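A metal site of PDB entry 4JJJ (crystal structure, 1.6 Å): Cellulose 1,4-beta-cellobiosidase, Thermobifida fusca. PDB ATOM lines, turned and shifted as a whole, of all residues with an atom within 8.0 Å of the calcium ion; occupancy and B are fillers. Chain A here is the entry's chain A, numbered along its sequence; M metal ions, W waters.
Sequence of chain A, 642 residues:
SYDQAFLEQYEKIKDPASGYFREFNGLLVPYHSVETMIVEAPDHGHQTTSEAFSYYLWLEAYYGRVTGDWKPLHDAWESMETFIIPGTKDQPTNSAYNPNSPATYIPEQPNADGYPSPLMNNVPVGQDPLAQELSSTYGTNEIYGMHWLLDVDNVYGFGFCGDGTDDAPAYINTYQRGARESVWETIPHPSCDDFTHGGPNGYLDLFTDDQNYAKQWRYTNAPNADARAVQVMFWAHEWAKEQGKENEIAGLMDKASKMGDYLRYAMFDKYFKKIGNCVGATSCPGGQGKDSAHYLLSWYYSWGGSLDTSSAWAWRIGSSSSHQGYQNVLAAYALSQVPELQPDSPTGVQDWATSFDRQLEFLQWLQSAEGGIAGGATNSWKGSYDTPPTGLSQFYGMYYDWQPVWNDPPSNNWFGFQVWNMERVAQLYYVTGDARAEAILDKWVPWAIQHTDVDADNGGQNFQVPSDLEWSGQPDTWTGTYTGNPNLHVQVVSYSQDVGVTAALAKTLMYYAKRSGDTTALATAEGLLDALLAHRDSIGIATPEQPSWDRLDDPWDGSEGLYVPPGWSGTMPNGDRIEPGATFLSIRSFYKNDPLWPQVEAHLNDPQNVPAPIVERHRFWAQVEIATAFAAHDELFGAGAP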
ATOM      1  N   PRO A 110      11.802   1.748 -21.305  1.00  0.00           N
ATOM      2  CA  PRO A 110      12.545   2.113 -22.539  1.00  0.00           C
ATOM      3  C   PRO A 110      14.067   2.279 -22.430  1.00  0.00           C
ATOM      4  O   PRO A 110      14.783   2.121 -23.463  1.00  0.00           O
ATOM      5  CB  PRO A 110      11.903   3.425 -22.935  1.00  0.00           C
ATOM      6  CG  PRO A 110      10.816   3.753 -21.983  1.00  0.00           C
ATOM      7  CD  PRO A 110      10.752   2.708 -20.920  1.00  0.00           C
ATOM      8  N   ASN A 111      14.571   2.543 -21.220  1.00  0.00           N
ATOM      9  CA  ASN A 111      15.980   2.600 -20.979  1.00  0.00           C
ATOM     10  C   ASN A 111      16.261   2.105 -19.561  1.00  0.00           C
ATOM     11  O   ASN A 111      15.363   1.825 -18.767  1.00  0.00           O
ATOM     12  CB  ASN A 111      16.527   4.017 -21.232  1.00  0.00           C
ATOM     13  CG  ASN A 111      17.960   4.077 -21.657  1.00  0.00           C
ATOM     14  OD1 ASN A 111      18.684   3.048 -21.633  1.00  0.00           O
ATOM     15  ND2 ASN A 111      18.429   5.254 -22.123  1.00  0.00           N
ATOM     16  N   ALA A 112      17.537   1.833 -19.302  1.00  0.00           N
ATOM     17  CA  ALA A 112      18.015   1.234 -18.051  1.00  0.00           C
ATOM     18  C   ALA A 112      17.640   2.039 -16.787  1.00  0.00           C
ATOM     19  O   ALA A 112      17.392   1.455 -15.726  1.00  0.00           O
ATOM     20  CB  ALA A 112      19.543   1.073 -18.145  1.00  0.00           C
ATOM     21  N   GLY A 178      16.078  -4.216 -20.278  1.00  0.00           N
ATOM     22  CA  GLY A 178      15.356  -3.817 -21.480  1.00  0.00           C
ATOM     23  C   GLY A 178      16.198  -3.631 -22.739  1.00  0.00           C
ATOM     24  O   GLY A 178      17.421  -4.005 -22.824  1.00  0.00           O
ATOM     25  N   ALA A 179      15.561  -3.148 -23.780  1.00  0.00           N
ATOM     26  CA  ALA A 179      16.136  -3.077 -25.056  1.00  0.00           C
ATOM     27  C   ALA A 179      17.360  -2.277 -25.267  1.00  0.00           C
ATOM     28  O   ALA A 179      18.116  -2.482 -26.213  1.00  0.00           O
ATOM     29  CB  ALA A 179      15.076  -2.631 -26.087  1.00  0.00           C
ATOM     30  N   ARG A 180      17.575  -1.280 -24.399  1.00  0.00           N
ATOM     31  CA  ARG A 180      18.662  -0.353 -24.596  1.00  0.00           C
ATOM     32  C   ARG A 180      19.813  -0.719 -23.722  1.00  0.00           C
ATOM     33  O   ARG A 180      20.779  -0.010 -23.694  1.00  0.00           O
ATOM     34  CB  ARG A 180      18.150   1.102 -24.312  1.00  0.00           C
ATOM     35  CG  ARG A 180      17.347   1.619 -25.499  1.00  0.00           C
ATOM     36  CD  ARG A 180      17.095   3.131 -25.382  1.00  0.00           C
ATOM     37  NE  ARG A 180      18.280   3.912 -25.451  1.00  0.00           N
ATOM     38  CZ  ARG A 180      18.292   5.254 -25.443  1.00  0.00           C
ATOM     39  NH1 ARG A 180      17.137   5.926 -25.394  1.00  0.00           N
ATOM     40  NH2 ARG A 180      19.446   5.920 -25.481  1.00  0.00           N
ATOM     41  N   GLU A 181      19.703  -1.802 -22.988  1.00  0.00           N
ATOM     42  CA  GLU A 181      20.824  -2.190 -22.110  1.00  0.00           C
ATOM     43  C   GLU A 181      21.731  -3.146 -22.961  1.00  0.00           C
ATOM     44  O   GLU A 181      21.418  -4.336 -23.099  1.00  0.00           O
ATOM     45  CB  GLU A 181      20.321  -2.888 -20.855  1.00  0.00           C
ATOM     46  CG  GLU A 181      21.427  -3.283 -19.903  1.00  0.00           C
ATOM     47  CD  GLU A 181      21.010  -4.214 -18.835  1.00  0.00           C
ATOM     48  OE1 GLU A 181      20.264  -5.229 -19.106  1.00  0.00           O
ATOM     49  OE2 GLU A 181      21.270  -3.951 -17.595  1.00  0.00           O
ATOM     50  N   SER A 182      22.854  -2.615 -23.446  1.00  0.00           N
ATOM     51  CA  SER A 182      23.825  -3.407 -24.176  1.00  0.00           C
ATOM     52  C   SER A 182      24.714  -4.261 -23.223  1.00  0.00           C
ATOM     53  O   SER A 182      24.615  -4.207 -21.997  1.00  0.00           O
ATOM     54  CB  SER A 182      24.683  -2.486 -24.906  1.00  0.00           C
ATOM     55  OG  SER A 182      25.725  -1.921 -24.070  1.00  0.00           O
ATOM     56  N   VAL A 183      25.529  -5.113 -23.861  1.00  0.00           N
ATOM     57  CA  VAL A 183      26.531  -5.950 -23.122  1.00  0.00           C
ATOM     58  C   VAL A 183      27.395  -5.105 -22.230  1.00  0.00           C
ATOM     59  O   VAL A 183      27.939  -5.552 -21.203  1.00  0.00           O
ATOM     60  CB  VAL A 183      27.355  -6.753 -24.174  1.00  0.00           C
ATOM     61  CG1 VAL A 183      28.145  -5.808 -25.069  1.00  0.00           C
ATOM     62  CG2 VAL A 183      28.178  -7.836 -23.485  1.00  0.00           C
ATOM     63  N   TRP A 184      27.589  -3.813 -22.604  1.00  0.00           N
ATOM     64  CA  TRP A 184      28.464  -2.860 -21.852  1.00  0.00           C
ATOM     65  C   TRP A 184      27.773  -2.278 -20.634  1.00  0.00           C
ATOM     66  O   TRP A 184      28.458  -1.648 -19.842  1.00  0.00           O
ATOM     67  CB  TRP A 184      28.894  -1.737 -22.748  1.00  0.00           C
ATOM     68  CG  TRP A 184      29.614  -2.176 -23.938  1.00  0.00           C
ATOM     69  CD1 TRP A 184      29.065  -2.471 -25.153  1.00  0.00           C
ATOM     70  CD2 TRP A 184      30.959  -2.621 -23.977  1.00  0.00           C
ATOM     71  NE1 TRP A 184      30.061  -2.976 -26.005  1.00  0.00           N
ATOM     72  CE2 TRP A 184      31.224  -3.072 -25.299  1.00  0.00           C
ATOM     73  CE3 TRP A 184      31.993  -2.595 -23.060  1.00  0.00           C
ATOM     74  CZ2 TRP A 184      32.493  -3.577 -25.661  1.00  0.00           C
ATOM     75  CZ3 TRP A 184      33.238  -3.078 -23.427  1.00  0.00           C
ATOM     76  CH2 TRP A 184      33.483  -3.523 -24.701  1.00  0.00           C
ATOM     77  N   GLU A 185      26.445  -2.462 -20.507  1.00  0.00           N
ATOM     78  CA  GLU A 185      25.606  -1.688 -19.571  1.00  0.00           C
ATOM     79  C   GLU A 185      24.921  -2.501 -18.527  1.00  0.00           C
ATOM     80  O   GLU A 185      24.089  -1.983 -17.819  1.00  0.00           O
ATOM     81  CB  GLU A 185      24.613  -0.848 -20.389  1.00  0.00           C
ATOM     82  CG  GLU A 185      25.263   0.260 -21.261  1.00  0.00           C
ATOM     83  CD  GLU A 185      24.362   0.825 -22.298  1.00  0.00           C
ATOM     84  OE1 GLU A 185      23.690   0.069 -22.970  1.00  0.00           O
ATOM     85  OE2 GLU A 185      24.330   2.029 -22.506  1.00  0.00           O
ATOM     86  N   ASN A 407      18.191  -3.463 -28.901  1.00  0.00           N
ATOM     87  CA  ASN A 407      18.346  -2.280 -29.777  1.00  0.00           C
ATOM     88  C   ASN A 407      19.716  -1.581 -29.662  1.00  0.00           C
ATOM     89  O   ASN A 407      20.000  -0.594 -30.244  1.00  0.00           O
ATOM     90  CB  ASN A 407      17.305  -1.266 -29.374  1.00  0.00           C
ATOM     91  CG  ASN A 407      15.838  -1.652 -29.549  1.00  0.00           C
ATOM     92  OD1 ASN A 407      14.932  -0.830 -29.113  1.00  0.00           O
ATOM     93  ND2 ASN A 407      15.538  -2.750 -30.148  1.00  0.00           N
ATOM     94  N   ASP A 408      20.592  -2.173 -28.832  1.00  0.00           N
ATOM     95  CA  ASP A 408      21.983  -1.723 -28.601  1.00  0.00           C
ATOM     96  C   ASP A 408      22.936  -2.889 -28.638  1.00  0.00           C
ATOM     97  O   ASP A 408      23.385  -3.313 -27.590  1.00  0.00           O
ATOM     98  CB  ASP A 408      22.023  -0.951 -27.267  1.00  0.00           C
ATOM     99  CG  ASP A 408      23.309  -0.161 -27.066  1.00  0.00           C
ATOM    100  OD1 ASP A 408      23.310   0.525 -26.007  1.00  0.00           O
ATOM    101  OD2 ASP A 408      24.179  -0.168 -27.919  1.00  0.00           O
ATOM    102  N   PRO A 409      23.286  -3.361 -29.843  1.00  0.00           N
ATOM    103  CA  PRO A 409      22.925  -2.913 -31.157  1.00  0.00           C
ATOM    104  C   PRO A 409      21.606  -3.553 -31.635  1.00  0.00           C
ATOM    105  O   PRO A 409      21.167  -4.545 -31.119  1.00  0.00           O
ATOM    106  CB  PRO A 409      24.075  -3.450 -31.991  1.00  0.00           C
ATOM    107  CG  PRO A 409      24.366  -4.767 -31.394  1.00  0.00           C
ATOM    108  CD  PRO A 409      24.251  -4.497 -29.909  1.00  0.00           C
ATOM    109  N   ARG A 551      33.470   1.943 -24.892  1.00  0.00           N
ATOM    110  CA  ARG A 551      32.440   2.023 -23.836  1.00  0.00           C
ATOM    111  C   ARG A 551      32.850   1.464 -22.474  1.00  0.00           C
ATOM    112  O   ARG A 551      32.103   1.544 -21.508  1.00  0.00           O
ATOM    113  CB  ARG A 551      31.205   1.257 -24.326  1.00  0.00           C
ATOM    114  CG  ARG A 551      30.685   1.801 -25.627  1.00  0.00           C
ATOM    115  CD  ARG A 551      29.534   1.048 -26.303  1.00  0.00           C
ATOM    116  NE  ARG A 551      28.348   1.147 -25.457  1.00  0.00           N
ATOM    117  CZ  ARG A 551      27.093   0.857 -25.866  1.00  0.00           C
ATOM    118  NH1 ARG A 551      26.874   0.278 -27.059  1.00  0.00           N
ATOM    119  NH2 ARG A 551      26.089   1.034 -25.046  1.00  0.00           N
ATOM    120  N   TRP A 556      27.098   6.467 -16.800  1.00  0.00           N
ATOM    121  CA  TRP A 556      25.779   6.873 -17.306  1.00  0.00           C
ATOM    122  C   TRP A 556      25.790   8.370 -17.566  1.00  0.00           C
ATOM    123  O   TRP A 556      26.317   9.154 -16.714  1.00  0.00           O
ATOM    124  CB  TRP A 556      24.748   6.618 -16.205  1.00  0.00           C
ATOM    125  CG  TRP A 556      23.397   7.079 -16.482  1.00  0.00           C
ATOM    126  CD1 TRP A 556      22.740   8.105 -15.816  1.00  0.00           C
ATOM    127  CD2 TRP A 556      22.409   6.503 -17.390  1.00  0.00           C
ATOM    128  NE1 TRP A 556      21.465   8.207 -16.272  1.00  0.00           N
ATOM    129  CE2 TRP A 556      21.266   7.297 -17.288  1.00  0.00           C
ATOM    130  CE3 TRP A 556      22.437   5.524 -18.386  1.00  0.00           C
ATOM    131  CZ2 TRP A 556      20.134   7.026 -17.988  1.00  0.00           C
ATOM    132  CZ3 TRP A 556      21.308   5.297 -19.133  1.00  0.00           C
ATOM    133  CH2 TRP A 556      20.146   5.991 -18.886  1.00  0.00           C
ATOM    134  N   SER A 559      21.612   8.752 -21.025  1.00  0.00           N
ATOM    135  CA  SER A 559      21.039   7.835 -22.034  1.00  0.00           C
ATOM    136  C   SER A 559      21.870   6.597 -22.293  1.00  0.00           C
ATOM    137  O   SER A 559      21.264   5.579 -22.615  1.00  0.00           O
ATOM    138  CB  SER A 559      20.790   8.511 -23.340  1.00  0.00           C
ATOM    139  OG  SER A 559      21.919   9.097 -23.763  1.00  0.00           O
ATOM    140  N   GLU A 560      23.207   6.698 -22.148  1.00  0.00           N
ATOM    141  CA  GLU A 560      24.127   5.584 -22.412  1.00  0.00           C
ATOM    142  C   GLU A 560      25.088   5.450 -21.251  1.00  0.00           C
ATOM    143  O   GLU A 560      25.396   6.443 -20.525  1.00  0.00           O
ATOM    144  CB  GLU A 560      24.820   5.747 -23.732  1.00  0.00           C
ATOM    145  CG  GLU A 560      23.880   5.984 -24.918  1.00  0.00           C
ATOM    146  CD  GLU A 560      23.079   4.747 -25.291  1.00  0.00           C
ATOM    147  OE1 GLU A 560      23.426   3.658 -24.830  1.00  0.00           O
ATOM    148  OE2 GLU A 560      22.096   4.943 -26.061  1.00  0.00           O
ATOM    149  N   GLY A 561      25.693   4.250 -21.109  1.00  0.00           N
ATOM    150  CA  GLY A 561      26.647   3.975 -20.033  1.00  0.00           C
ATOM    151  C   GLY A 561      26.013   3.226 -18.921  1.00  0.00           C
ATOM    152  O   GLY A 561      24.798   2.958 -18.934  1.00  0.00           O
ATOM    153  N   LEU A 562      26.780   2.894 -17.894  1.00  0.00           N
ATOM    154  CA  LEU A 562      26.289   2.035 -16.818  1.00  0.00           C
ATOM    155  C   LEU A 562      25.420   2.783 -15.853  1.00  0.00           C
ATOM    156  O   LEU A 562      25.898   3.729 -15.181  1.00  0.00           O
ATOM    157  CB  LEU A 562      27.487   1.429 -16.063  1.00  0.00           C
ATOM    158  CG  LEU A 562      27.112   0.559 -14.886  1.00  0.00           C
ATOM    159  CD1 LEU A 562      26.075  -0.519 -15.227  1.00  0.00           C
ATOM    160  CD2 LEU A 562      28.351   0.039 -14.274  1.00  0.00           C
HETATM  161 CA    CA M   1      22.408   1.621 -24.236  1.00  0.00          CA
HETATM  162  O   HOH W   1      21.258   2.926 -22.668  1.00  0.00           O
HETATM  163  O   HOH W   2      20.852   2.539 -25.975  1.00  0.00           O
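Arg 551 touches the calcium ion (NH2 to CA, 3.8 Å). Within 4 Å of the calcium ion: Arg 180, Glu 185, Asp 408, Arg 551 and Glu 560. Along chain A the residues within 4 Å of the calcium ion span positions 180 to 560. The nearest printed residue that does not touch the calcium ion is Ser 182 (4.3 Å).
The calcium ion is bound by the side-chain carboxylate (OD1) of Asp 408 (2.3 Å), water W1 (2.3 Å), the side-chain carboxylate (OE1) of Glu 560 (2.4 Å), the backbone carbonyl oxygen (O) of Arg 180 (2.4 Å), the side-chain carboxylate (OE1) of Glu 185 (2.4 Å), water W2 (2.5 Å) and the side-chain carboxylate (OE2) of Glu 185 (2.6 Å). The calcium ion has seven donor atoms within binding distance.
N of Gly 561 sits close to OE2 of Glu 185 (3.0 Å). The side-chain hydroxyl of Ser 182 is in hydrogen-bond range of the guanidinium group of Arg 551, 3.1 Å away. NH2 of Arg 180 is in hydrogen-bond range of O of Ser 559 (3.4 Å). OD2 of Asp 408 lies within salt-bridge range of NH1 of Arg 551 (2.9 Å). NH2 of Arg 551 sits close to OE2 of Glu 185 (3.2 Å). The side-chain carboxylate (OE1) of Glu 185 lies close to the backbone NH (N) of Ser 182, 2.9 Å away. OE1 of Glu 560 lies close to NH2 of Arg 551.
Water W2 lies within hydrogen-bond range of the side-chain carboxylate of Glu 560 and the guanidinium group of Arg 180. Water W1 lies within hydrogen-bond range of the backbone carbonyl oxygen of Ser 559 and the side-chain amide oxygen of Asn 111.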
